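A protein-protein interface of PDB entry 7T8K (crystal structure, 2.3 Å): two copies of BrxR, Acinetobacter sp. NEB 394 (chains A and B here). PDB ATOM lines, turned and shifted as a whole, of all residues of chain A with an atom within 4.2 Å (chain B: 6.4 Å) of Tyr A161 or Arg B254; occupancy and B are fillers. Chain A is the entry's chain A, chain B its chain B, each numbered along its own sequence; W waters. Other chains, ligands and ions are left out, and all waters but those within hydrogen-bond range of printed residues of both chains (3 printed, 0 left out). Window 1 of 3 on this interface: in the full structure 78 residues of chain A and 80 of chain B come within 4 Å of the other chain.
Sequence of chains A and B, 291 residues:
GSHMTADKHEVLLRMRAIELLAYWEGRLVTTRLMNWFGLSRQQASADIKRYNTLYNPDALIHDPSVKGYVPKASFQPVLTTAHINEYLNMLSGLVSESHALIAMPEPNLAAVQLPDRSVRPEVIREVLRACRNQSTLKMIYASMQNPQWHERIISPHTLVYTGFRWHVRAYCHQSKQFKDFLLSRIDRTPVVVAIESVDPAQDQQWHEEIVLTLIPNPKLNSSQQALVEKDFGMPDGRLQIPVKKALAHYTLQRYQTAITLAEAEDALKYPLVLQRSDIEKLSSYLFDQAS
ND2 of Asn B85 sits at hydrogen-bond distance from O of Leu A114 (3.3 Å).
The backbone carbonyl oxygen of Ala B110 is in hydrogen-bond range of the backbone NH of Tyr A161 (2.9 Å).
N of Val B112 is in hydrogen-bond range of O of Tyr A161 (2.7 Å).
The backbone carbonyl oxygen (O) of Gly A163 sits at hydrogen-bond distance from the guanidinium group (NH1) of Arg B254.
Among the printed residues, merely in contact across the chains: Val A112 with Thr B162 (3.7 Å), Val A112 with Arg B254 (3.7 Å), Gln A113 with Arg B254 (3.9 Å), Leu A114 with Arg B254 (3.7 Å), Leu A114 with Tyr B255 (3.2 Å), Val A160 with Ala B110 (3.3 Å), Tyr A161 with Leu B88 (3.6 Å), Tyr A161 with Ala B111 (3.3 Å), Tyr A161 with Arg B254 (3.8 Å), Thr A162 with Val B112 (3.6 Å), Phe A164 with Phe B164 (3.8 Å), Phe A164 with Arg B254 (3.4 Å), Phe A164 with Gln B256 (3.3 Å), Trp A166 with Ile B84 (3.3 Å), Trp A166 with Leu B88 (3.6 Å) and Trp A166 with Leu B109 (3.96 Å).
Water W1 lies within hydrogen-bond range of O of Val A112 (2.7 Å) and NE of Arg B254 (2.9 Å).
Water W3 bridges NE of Arg A165 (2.8 Å) and OE1 of Gln B256 (2.9 Å).
Water W2 bridges the indole nitrogen of Trp A166 and the side-chain amide oxygen of Asn B85.
Hydrophobic or aromatic side chains of chain A that line the printed part of chain B: Val A112, Leu A114, Tyr A161, Phe A164 and Trp A166.
Of the 20 printed residues of chain B, 12 touch a printed residue of chain A.
Among the printed residues, 20 pairs touch across the chains.
Among the printed residues, no Asp or Glu carboxylate lies within 4 Å of a Lys or Arg side-chain nitrogen of the other chain.
Of the printed residues of chain B, Leu A114 touches Asn B85 (3.3 Å), Arg B254 (3.7 Å) and Tyr B255 (3.2 Å).
Of chain B, only Leu B88, Ala B110, Ala B111, Val B112 and Arg B254 come within 4 Å of Tyr A161.
Printed residues of chain A within 4 Å of Leu B88: Tyr A161 (3.6 Å) and Trp A166 (3.6 Å).
Of the printed residues of chain A, Leu B109 touches Trp A166.
Of the printed residues of chain A, Thr B162 touches Val A112.
Gly B163 touches none of the printed residues of chain A.
Arg B254 touches six residues of chain A.
Thr B257 touches none of the printed residues of chain A.
The nearest residue of chain B that does not touch Tyr A161 is Asn B85 (5.2 Å).
The side-chain hydroxyl of Tyr A161 lies within hydrogen-bond range of the backbone carbonyl oxygen of Gly A163, 3.5 Å away.
The side-chain hydroxyl (OG1) of Thr A162 lies within hydrogen-bond range of the backbone NH (N) of Phe A164 (3.0 Å).
OG1 of Thr A162 is in hydrogen-bond range of N of Arg A165 (2.9 Å).
The side-chain hydroxyl (OG1) of Thr B162 is in hydrogen-bond range of the backbone NH (N) of Phe B164, 3.2 Å away.
Val A112 touches Thr B162, and with the chains exchanged Thr A162 touches Val B112.
Phe B164 touches its own counterpart, Phe A164.
Positions printed for both chains: 112, 113, 162, 163 and 164.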
ATOM      1  N   VAL A 112      -3.683  14.589 -28.512  1.00  0.00           N
ATOM      2  CA  VAL A 112      -2.624  15.018 -27.608  1.00  0.00           C
ATOM      3  C   VAL A 112      -1.340  14.285 -27.966  1.00  0.00           C
ATOM      4  O   VAL A 112      -1.339  13.062 -28.162  1.00  0.00           O
ATOM      5  CB  VAL A 112      -3.028  14.759 -26.151  1.00  0.00           C
ATOM      6  CG1 VAL A 112      -1.873  15.064 -25.216  1.00  0.00           C
ATOM      7  CG2 VAL A 112      -4.240  15.582 -25.794  1.00  0.00           C
ATOM      8  N   GLN A 113      -0.240  15.028 -28.069  1.00  0.00           N
ATOM      9  CA  GLN A 113       1.042  14.459 -28.455  1.00  0.00           C
ATOM     10  C   GLN A 113       2.095  14.809 -27.414  1.00  0.00           C
ATOM     11  O   GLN A 113       1.893  15.665 -26.548  1.00  0.00           O
ATOM     12  CB  GLN A 113       1.484  14.944 -29.841  1.00  0.00           C
ATOM     13  CG  GLN A 113       0.489  14.647 -30.945  1.00  0.00           C
ATOM     14  CD  GLN A 113       1.088  14.803 -32.329  1.00  0.00           C
ATOM     15  OE1 GLN A 113       0.859  13.977 -33.209  1.00  0.00           O
ATOM     16  NE2 GLN A 113       1.860  15.865 -32.528  1.00  0.00           N
ATOM     17  N   LEU A 114       3.234  14.126 -27.502  1.00  0.00           N
ATOM     18  CA  LEU A 114       4.388  14.405 -26.651  1.00  0.00           C
ATOM     19  C   LEU A 114       5.588  14.634 -27.558  1.00  0.00           C
ATOM     20  O   LEU A 114       6.327  13.694 -27.887  1.00  0.00           O
ATOM     21  CB  LEU A 114       4.639  13.271 -25.661  1.00  0.00           C
ATOM     22  CG  LEU A 114       5.824  13.499 -24.724  1.00  0.00           C
ATOM     23  CD1 LEU A 114       5.645  14.807 -23.995  1.00  0.00           C
ATOM     24  CD2 LEU A 114       5.962  12.353 -23.736  1.00  0.00           C
ATOM     25  N   VAL A 160      14.542   1.762 -27.534  1.00  0.00           N
ATOM     26  CA  VAL A 160      13.214   1.577 -26.967  1.00  0.00           C
ATOM     27  C   VAL A 160      12.527   2.929 -26.850  1.00  0.00           C
ATOM     28  O   VAL A 160      13.067   3.858 -26.238  1.00  0.00           O
ATOM     29  CB  VAL A 160      13.273   0.888 -25.588  1.00  0.00           C
ATOM     30  CG1 VAL A 160      11.872   0.698 -25.027  1.00  0.00           C
ATOM     31  CG2 VAL A 160      14.004  -0.448 -25.682  1.00  0.00           C
ATOM     32  N   TYR A 161      11.333   3.025 -27.419  1.00  0.00           N
ATOM     33  CA  TYR A 161      10.424   4.138 -27.183  1.00  0.00           C
ATOM     34  C   TYR A 161       9.318   3.625 -26.276  1.00  0.00           C
ATOM     35  O   TYR A 161       8.581   2.709 -26.654  1.00  0.00           O
ATOM     36  CB  TYR A 161       9.845   4.676 -28.490  1.00  0.00           C
ATOM     37  CG  TYR A 161       8.852   5.802 -28.303  1.00  0.00           C
ATOM     38  CD1 TYR A 161       9.239   7.005 -27.728  1.00  0.00           C
ATOM     39  CD2 TYR A 161       7.532   5.662 -28.699  1.00  0.00           C
ATOM     40  CE1 TYR A 161       8.337   8.042 -27.559  1.00  0.00           C
ATOM     41  CE2 TYR A 161       6.618   6.693 -28.533  1.00  0.00           C
ATOM     42  CZ  TYR A 161       7.027   7.881 -27.962  1.00  0.00           C
ATOM     43  OH  TYR A 161       6.126   8.910 -27.796  1.00  0.00           O
ATOM     44  N   THR A 162       9.213   4.209 -25.086  1.00  0.00           N
ATOM     45  CA  THR A 162       8.257   3.774 -24.080  1.00  0.00           C
ATOM     46  C   THR A 162       6.888   4.414 -24.239  1.00  0.00           C
ATOM     47  O   THR A 162       5.963   4.042 -23.509  1.00  0.00           O
ATOM     48  CB  THR A 162       8.780   4.106 -22.681  1.00  0.00           C
ATOM     49  OG1 THR A 162       8.725   5.528 -22.484  1.00  0.00           O
ATOM     50  CG2 THR A 162      10.214   3.636 -22.528  1.00  0.00           C
ATOM     51  N   GLY A 163       6.734   5.345 -25.177  1.00  0.00           N
ATOM     52  CA  GLY A 163       5.601   6.239 -25.193  1.00  0.00           C
ATOM     53  C   GLY A 163       5.832   7.528 -24.437  1.00  0.00           C
ATOM     54  O   GLY A 163       5.001   8.443 -24.525  1.00  0.00           O
ATOM     55  N   PHE A 164       6.928   7.626 -23.688  1.00  0.00           N
ATOM     56  CA  PHE A 164       7.252   8.857 -22.982  1.00  0.00           C
ATOM     57  C   PHE A 164       8.712   9.231 -23.185  1.00  0.00           C
ATOM     58  O   PHE A 164       9.044  10.414 -23.295  1.00  0.00           O
ATOM     59  CB  PHE A 164       6.940   8.710 -21.490  1.00  0.00           C
ATOM     60  CG  PHE A 164       5.539   8.254 -21.212  1.00  0.00           C
ATOM     61  CD1 PHE A 164       4.500   9.172 -21.144  1.00  0.00           C
ATOM     62  CD2 PHE A 164       5.253   6.911 -21.032  1.00  0.00           C
ATOM     63  CE1 PHE A 164       3.198   8.758 -20.891  1.00  0.00           C
ATOM     64  CE2 PHE A 164       3.956   6.488 -20.779  1.00  0.00           C
ATOM     65  CZ  PHE A 164       2.926   7.413 -20.710  1.00  0.00           C
ATOM     66  N   ARG A 165       9.587   8.233 -23.263  1.00  0.00           N
ATOM     67  CA  ARG A 165      11.015   8.486 -23.343  1.00  0.00           C
ATOM     68  C   ARG A 165      11.669   7.462 -24.251  1.00  0.00           C
ATOM     69  O   ARG A 165      11.134   6.377 -24.495  1.00  0.00           O
ATOM     70  CB  ARG A 165      11.679   8.425 -21.960  1.00  0.00           C
ATOM     71  CG  ARG A 165      11.079   9.356 -20.930  1.00  0.00           C
ATOM     72  CD  ARG A 165      11.776   9.169 -19.591  1.00  0.00           C
ATOM     73  NE  ARG A 165      11.263  10.078 -18.570  1.00  0.00           N
ATOM     74  CZ  ARG A 165      11.965  11.072 -18.040  1.00  0.00           C
ATOM     75  NH1 ARG A 165      13.215  11.285 -18.435  1.00  0.00           N
ATOM     76  NH2 ARG A 165      11.426  11.848 -17.112  1.00  0.00           N
ATOM     77  N   TRP A 166      12.856   7.812 -24.725  1.00  0.00           N
ATOM     78  CA  TRP A 166      13.685   6.909 -25.502  1.00  0.00           C
ATOM     79  C   TRP A 166      14.848   6.460 -24.638  1.00  0.00           C
ATOM     80  O   TRP A 166      15.484   7.280 -23.971  1.00  0.00           O
ATOM     81  CB  TRP A 166      14.209   7.589 -26.767  1.00  0.00           C
ATOM     82  CG  TRP A 166      13.167   7.839 -27.798  1.00  0.00           C
ATOM     83  CD1 TRP A 166      12.264   8.860 -27.820  1.00  0.00           C
ATOM     84  CD2 TRP A 166      12.922   7.057 -28.977  1.00  0.00           C
ATOM     85  NE1 TRP A 166      11.468   8.763 -28.939  1.00  0.00           N
ATOM     86  CE2 TRP A 166      11.853   7.665 -29.664  1.00  0.00           C
ATOM     87  CE3 TRP A 166      13.501   5.904 -29.513  1.00  0.00           C
ATOM     88  CZ2 TRP A 166      11.350   7.156 -30.861  1.00  0.00           C
ATOM     89  CZ3 TRP A 166      13.002   5.401 -30.700  1.00  0.00           C
ATOM     90  CH2 TRP A 166      11.938   6.027 -31.361  1.00  0.00           C
ATOM     91  N   ILE B  84      12.820  13.302 -33.013  1.00  0.00           N
ATOM     92  CA  ILE B  84      12.940  11.884 -33.325  1.00  0.00           C
ATOM     93  C   ILE B  84      11.583  11.266 -33.637  1.00  0.00           C
ATOM     94  O   ILE B  84      11.523  10.190 -34.241  1.00  0.00           O
ATOM     95  CB  ILE B  84      13.647  11.127 -32.177  1.00  0.00           C
ATOM     96  CG1 ILE B  84      14.023   9.712 -32.622  1.00  0.00           C
ATOM     97  CG2 ILE B  84      12.767  11.071 -30.939  1.00  0.00           C
ATOM     98  CD1 ILE B  84      15.111   9.076 -31.777  1.00  0.00           C
ATOM     99  N   ASN B  85      10.485  11.923 -33.244  1.00  0.00           N
ATOM    100  CA  ASN B  85       9.157  11.454 -33.641  1.00  0.00           C
ATOM    101  C   ASN B  85       9.057  11.307 -35.155  1.00  0.00           C
ATOM    102  O   ASN B  85       8.420  10.374 -35.661  1.00  0.00           O
ATOM    103  CB  ASN B  85       8.070  12.416 -33.144  1.00  0.00           C
ATOM    104  CG  ASN B  85       8.255  12.831 -31.693  1.00  0.00           C
ATOM    105  OD1 ASN B  85       9.374  13.079 -31.240  1.00  0.00           O
ATOM    106  ND2 ASN B  85       7.148  12.917 -30.957  1.00  0.00           N
ATOM    107  N   LEU B  88      10.559   7.894 -36.141  1.00  0.00           N
ATOM    108  CA  LEU B  88       9.713   6.776 -35.738  1.00  0.00           C
ATOM    109  C   LEU B  88       8.438   6.711 -36.570  1.00  0.00           C
ATOM    110  O   LEU B  88       7.985   5.620 -36.930  1.00  0.00           O
ATOM    111  CB  LEU B  88       9.379   6.883 -34.249  1.00  0.00           C
ATOM    112  CG  LEU B  88       8.399   5.843 -33.704  1.00  0.00           C
ATOM    113  CD1 LEU B  88       8.883   4.435 -34.005  1.00  0.00           C
ATOM    114  CD2 LEU B  88       8.208   6.027 -32.214  1.00  0.00           C
ATOM    115  N   LEU B 109      14.728  -1.963 -32.728  1.00  0.00           N
ATOM    116  CA  LEU B 109      13.886  -0.870 -32.264  1.00  0.00           C
ATOM    117  C   LEU B 109      12.565  -1.436 -31.777  1.00  0.00           C
ATOM    118  O   LEU B 109      11.843  -2.080 -32.544  1.00  0.00           O
ATOM    119  CB  LEU B 109      13.659   0.172 -33.358  1.00  0.00           C
ATOM    120  CG  LEU B 109      12.560   1.164 -32.976  1.00  0.00           C
ATOM    121  CD1 LEU B 109      12.892   2.561 -33.460  1.00  0.00           C
ATOM    122  CD2 LEU B 109      11.238   0.709 -33.534  1.00  0.00           C
ATOM    123  N   ALA B 110      12.242  -1.170 -30.517  1.00  0.00           N
ATOM    124  CA  ALA B 110      10.973  -1.554 -29.922  1.00  0.00           C
ATOM    125  C   ALA B 110      10.238  -0.294 -29.497  1.00  0.00           C
ATOM    126  O   ALA B 110      10.858   0.681 -29.065  1.00  0.00           O
ATOM    127  CB  ALA B 110      11.172  -2.484 -28.717  1.00  0.00           C
ATOM    128  N   ALA B 111       8.917  -0.306 -29.641  1.00  0.00           N
ATOM    129  CA  ALA B 111       8.101   0.854 -29.310  1.00  0.00           C
ATOM    130  C   ALA B 111       6.884   0.367 -28.547  1.00  0.00           C
ATOM    131  O   ALA B 111       6.064  -0.376 -29.094  1.00  0.00           O
ATOM    132  CB  ALA B 111       7.679   1.624 -30.564  1.00  0.00           C
ATOM    133  N   VAL B 112       6.780   0.777 -27.283  1.00  0.00           N
ATOM    134  CA  VAL B 112       5.625   0.418 -26.477  1.00  0.00           C
ATOM    135  C   VAL B 112       4.396   1.099 -27.056  1.00  0.00           C
ATOM    136  O   VAL B 112       4.417   2.298 -27.365  1.00  0.00           O
ATOM    137  CB  VAL B 112       5.845   0.813 -25.011  1.00  0.00           C
ATOM    138  CG1 VAL B 112       4.674   0.355 -24.160  1.00  0.00           C
ATOM    139  CG2 VAL B 112       7.153   0.229 -24.499  1.00  0.00           C
ATOM    140  N   GLN B 113       3.323   0.338 -27.221  1.00  0.00           N
ATOM    141  CA  GLN B 113       2.102   0.858 -27.810  1.00  0.00           C
ATOM    142  C   GLN B 113       0.942   0.597 -26.867  1.00  0.00           C
ATOM    143  O   GLN B 113       1.033  -0.204 -25.935  1.00  0.00           O
ATOM    144  CB  GLN B 113       1.820   0.221 -29.176  1.00  0.00           C
ATOM    145  CG  GLN B 113       2.800   0.601 -30.263  1.00  0.00           C
ATOM    146  CD  GLN B 113       2.369   0.106 -31.630  1.00  0.00           C
ATOM    147  OE1 GLN B 113       2.640   0.743 -32.646  1.00  0.00           O
ATOM    148  NE2 GLN B 113       1.690  -1.037 -31.659  1.00  0.00           N
ATOM    149  N   THR B 162      -6.394  11.343 -26.316  1.00  0.00           N
ATOM    150  CA  THR B 162      -5.555  11.861 -25.243  1.00  0.00           C
ATOM    151  C   THR B 162      -4.191  11.188 -25.183  1.00  0.00           C
ATOM    152  O   THR B 162      -3.354  11.584 -24.365  1.00  0.00           O
ATOM    153  CB  THR B 162      -6.251  11.701 -23.884  1.00  0.00           C
ATOM    154  OG1 THR B 162      -6.223  10.325 -23.486  1.00  0.00           O
ATOM    155  CG2 THR B 162      -7.698  12.175 -23.946  1.00  0.00           C
ATOM    156  N   GLY B 163      -3.945  10.185 -26.026  1.00  0.00           N
ATOM    157  CA  GLY B 163      -2.821   9.293 -25.844  1.00  0.00           C
ATOM    158  C   GLY B 163      -3.132   8.058 -25.031  1.00  0.00           C
ATOM    159  O   GLY B 163      -2.301   7.142 -24.981  1.00  0.00           O
ATOM    160  N   PHE B 164      -4.303   7.999 -24.400  1.00  0.00           N
ATOM    161  CA  PHE B 164      -4.719   6.828 -23.639  1.00  0.00           C
ATOM    162  C   PHE B 164      -6.149   6.430 -23.986  1.00  0.00           C
ATOM    163  O   PHE B 164      -6.485   5.242 -23.977  1.00  0.00           O
ATOM    164  CB  PHE B 164      -4.593   7.094 -22.134  1.00  0.00           C
ATOM    165  CG  PHE B 164      -3.242   7.595 -21.717  1.00  0.00           C
ATOM    166  CD1 PHE B 164      -2.226   6.706 -21.402  1.00  0.00           C
ATOM    167  CD2 PHE B 164      -2.984   8.954 -21.641  1.00  0.00           C
ATOM    168  CE1 PHE B 164      -0.979   7.163 -21.014  1.00  0.00           C
ATOM    169  CE2 PHE B 164      -1.738   9.418 -21.255  1.00  0.00           C
ATOM    170  CZ  PHE B 164      -0.734   8.522 -20.941  1.00  0.00           C
ATOM    171  N   HIS B 249      -5.623  18.915 -18.537  1.00  0.00           N
ATOM    172  CA  HIS B 249      -5.412  17.717 -17.728  1.00  0.00           C
ATOM    173  C   HIS B 249      -4.859  16.573 -18.569  1.00  0.00           C
ATOM    174  O   HIS B 249      -3.963  15.842 -18.131  1.00  0.00           O
ATOM    175  CB  HIS B 249      -6.717  17.312 -17.044  1.00  0.00           C
ATOM    176  CG  HIS B 249      -7.023  18.111 -15.815  1.00  0.00           C
ATOM    177  ND1 HIS B 249      -6.316  17.968 -14.641  1.00  0.00           N
ATOM    178  CD2 HIS B 249      -7.948  19.073 -15.584  1.00  0.00           C
ATOM    179  CE1 HIS B 249      -6.797  18.804 -13.736  1.00  0.00           C
ATOM    180  NE2 HIS B 249      -7.788  19.485 -14.283  1.00  0.00           N
ATOM    181  N   TYR B 250      -5.393  16.394 -19.778  1.00  0.00           N
ATOM    182  CA  TYR B 250      -4.877  15.357 -20.663  1.00  0.00           C
ATOM    183  C   TYR B 250      -3.408  15.589 -20.992  1.00  0.00           C
ATOM    184  O   TYR B 250      -2.614  14.645 -21.012  1.00  0.00           O
ATOM    185  CB  TYR B 250      -5.724  15.302 -21.930  1.00  0.00           C
ATOM    186  CG  TYR B 250      -7.174  15.048 -21.617  1.00  0.00           C
ATOM    187  CD1 TYR B 250      -7.553  13.930 -20.886  1.00  0.00           C
ATOM    188  CD2 TYR B 250      -8.160  15.932 -22.024  1.00  0.00           C
ATOM    189  CE1 TYR B 250      -8.878  13.691 -20.584  1.00  0.00           C
ATOM    190  CE2 TYR B 250      -9.494  15.702 -21.724  1.00  0.00           C
ATOM    191  CZ  TYR B 250      -9.845  14.579 -21.004  1.00  0.00           C
ATOM    192  OH  TYR B 250     -11.167  14.345 -20.704  1.00  0.00           O
ATOM    193  N   THR B 251      -3.036  16.836 -21.274  1.00  0.00           N
ATOM    194  CA  THR B 251      -1.639  17.166 -21.539  1.00  0.00           C
ATOM    195  C   THR B 251      -0.745  16.826 -20.348  1.00  0.00           C
ATOM    196  O   THR B 251       0.329  16.225 -20.506  1.00  0.00           O
ATOM    197  CB  THR B 251      -1.531  18.648 -21.900  1.00  0.00           C
ATOM    198  OG1 THR B 251      -2.312  18.905 -23.075  1.00  0.00           O
ATOM    199  CG2 THR B 251      -0.087  19.040 -22.161  1.00  0.00           C
ATOM    200  N   LEU B 252      -1.165  17.220 -19.142  1.00  0.00           N
ATOM    201  CA  LEU B 252      -0.366  16.919 -17.955  1.00  0.00           C
ATOM    202  C   LEU B 252      -0.203  15.416 -17.777  1.00  0.00           C
ATOM    203  O   LEU B 252       0.896  14.924 -17.477  1.00  0.00           O
ATOM    204  CB  LEU B 252      -1.006  17.549 -16.715  1.00  0.00           C
ATOM    205  CG  LEU B 252      -1.074  19.079 -16.702  1.00  0.00           C
ATOM    206  CD1 LEU B 252      -2.129  19.573 -15.722  1.00  0.00           C
ATOM    207  CD2 LEU B 252       0.284  19.670 -16.367  1.00  0.00           C
ATOM    208  N   GLN B 253      -1.287  14.662 -17.960  1.00  0.00           N
ATOM    209  CA  GLN B 253      -1.164  13.212 -17.896  1.00  0.00           C
ATOM    210  C   GLN B 253      -0.203  12.710 -18.963  1.00  0.00           C
ATOM    211  O   GLN B 253       0.618  11.823 -18.704  1.00  0.00           O
ATOM    212  CB  GLN B 253      -2.533  12.560 -18.065  1.00  0.00           C
ATOM    213  CG  GLN B 253      -3.086  11.968 -16.791  1.00  0.00           C
ATOM    214  CD  GLN B 253      -3.592  13.027 -15.840  1.00  0.00           C
ATOM    215  OE1 GLN B 253      -4.570  13.718 -16.125  1.00  0.00           O
ATOM    216  NE2 GLN B 253      -2.922  13.168 -14.700  1.00  0.00           N
ATOM    217  N   ARG B 254      -0.270  13.293 -20.166  1.00  0.00           N
ATOM    218  CA  ARG B 254       0.582  12.845 -21.261  1.00  0.00           C
ATOM    219  C   ARG B 254       2.046  13.026 -20.911  1.00  0.00           C
ATOM    220  O   ARG B 254       2.885  12.212 -21.306  1.00  0.00           O
ATOM    221  CB  ARG B 254       0.242  13.610 -22.542  1.00  0.00           C
ATOM    222  CG  ARG B 254       0.914  13.064 -23.789  1.00  0.00           C
ATOM    223  CD  ARG B 254       0.436  11.654 -24.090  1.00  0.00           C
ATOM    224  NE  ARG B 254       1.139  11.059 -25.222  1.00  0.00           N
ATOM    225  CZ  ARG B 254       2.283  10.391 -25.120  1.00  0.00           C
ATOM    226  NH1 ARG B 254       2.871  10.250 -23.938  1.00  0.00           N
ATOM    227  NH2 ARG B 254       2.852   9.878 -26.203  1.00  0.00           N
ATOM    228  N   TYR B 255       2.367  14.074 -20.157  1.00  0.00           N
ATOM    229  CA  TYR B 255       3.738  14.290 -19.712  1.00  0.00           C
ATOM    230  C   TYR B 255       4.063  13.555 -18.417  1.00  0.00           C
ATOM    231  O   TYR B 255       5.213  13.596 -17.971  1.00  0.00           O
ATOM    232  CB  TYR B 255       4.011  15.781 -19.523  1.00  0.00           C
ATOM    233  CG  TYR B 255       4.370  16.506 -20.795  1.00  0.00           C
ATOM    234  CD1 TYR B 255       5.671  16.932 -21.032  1.00  0.00           C
ATOM    235  CD2 TYR B 255       3.407  16.774 -21.758  1.00  0.00           C
ATOM    236  CE1 TYR B 255       6.002  17.603 -22.196  1.00  0.00           C
ATOM    237  CE2 TYR B 255       3.729  17.442 -22.922  1.00  0.00           C
ATOM    238  CZ  TYR B 255       5.027  17.855 -23.137  1.00  0.00           C
ATOM    239  OH  TYR B 255       5.349  18.522 -24.299  1.00  0.00           O
ATOM    240  N   GLN B 256       3.081  12.900 -17.797  1.00  0.00           N
ATOM    241  CA  GLN B 256       3.311  12.145 -16.564  1.00  0.00           C
ATOM    242  C   GLN B 256       3.702  13.070 -15.422  1.00  0.00           C
ATOM    243  O   GLN B 256       4.437  12.683 -14.511  1.00  0.00           O
ATOM    244  CB  GLN B 256       4.388  11.064 -16.751  1.00  0.00           C
ATOM    245  CG  GLN B 256       4.027   9.932 -17.714  1.00  0.00           C
ATOM    246  CD  GLN B 256       5.180   8.956 -17.942  1.00  0.00           C
ATOM    247  OE1 GLN B 256       6.317   9.363 -18.198  1.00  0.00           O
ATOM    248  NE2 GLN B 256       4.887   7.662 -17.857  1.00  0.00           N
ATOM    249  N   THR B 257       3.215  14.298 -15.475  1.00  0.00           N
ATOM    250  CA  THR B 257       3.589  15.313 -14.512  1.00  0.00           C
ATOM    251  C   THR B 257       2.744  15.184 -13.250  1.00  0.00           C
ATOM    252  O   THR B 257       1.572  14.805 -13.299  1.00  0.00           O
ATOM    253  CB  THR B 257       3.441  16.700 -15.139  1.00  0.00           C
ATOM    254  OG1 THR B 257       3.961  17.692 -14.244  1.00  0.00           O
ATOM    255  CG2 THR B 257       1.984  16.993 -15.441  1.00  0.00           C
HETATM  256  O   HOH W   1       0.076  10.730 -27.888  1.00  0.00           O
HETATM  257  O   HOH W   2       9.486  10.765 -29.500  1.00  0.00           O
HETATM  258  O   HOH W   3       9.034   8.426 -17.977  1.00  0.00           O
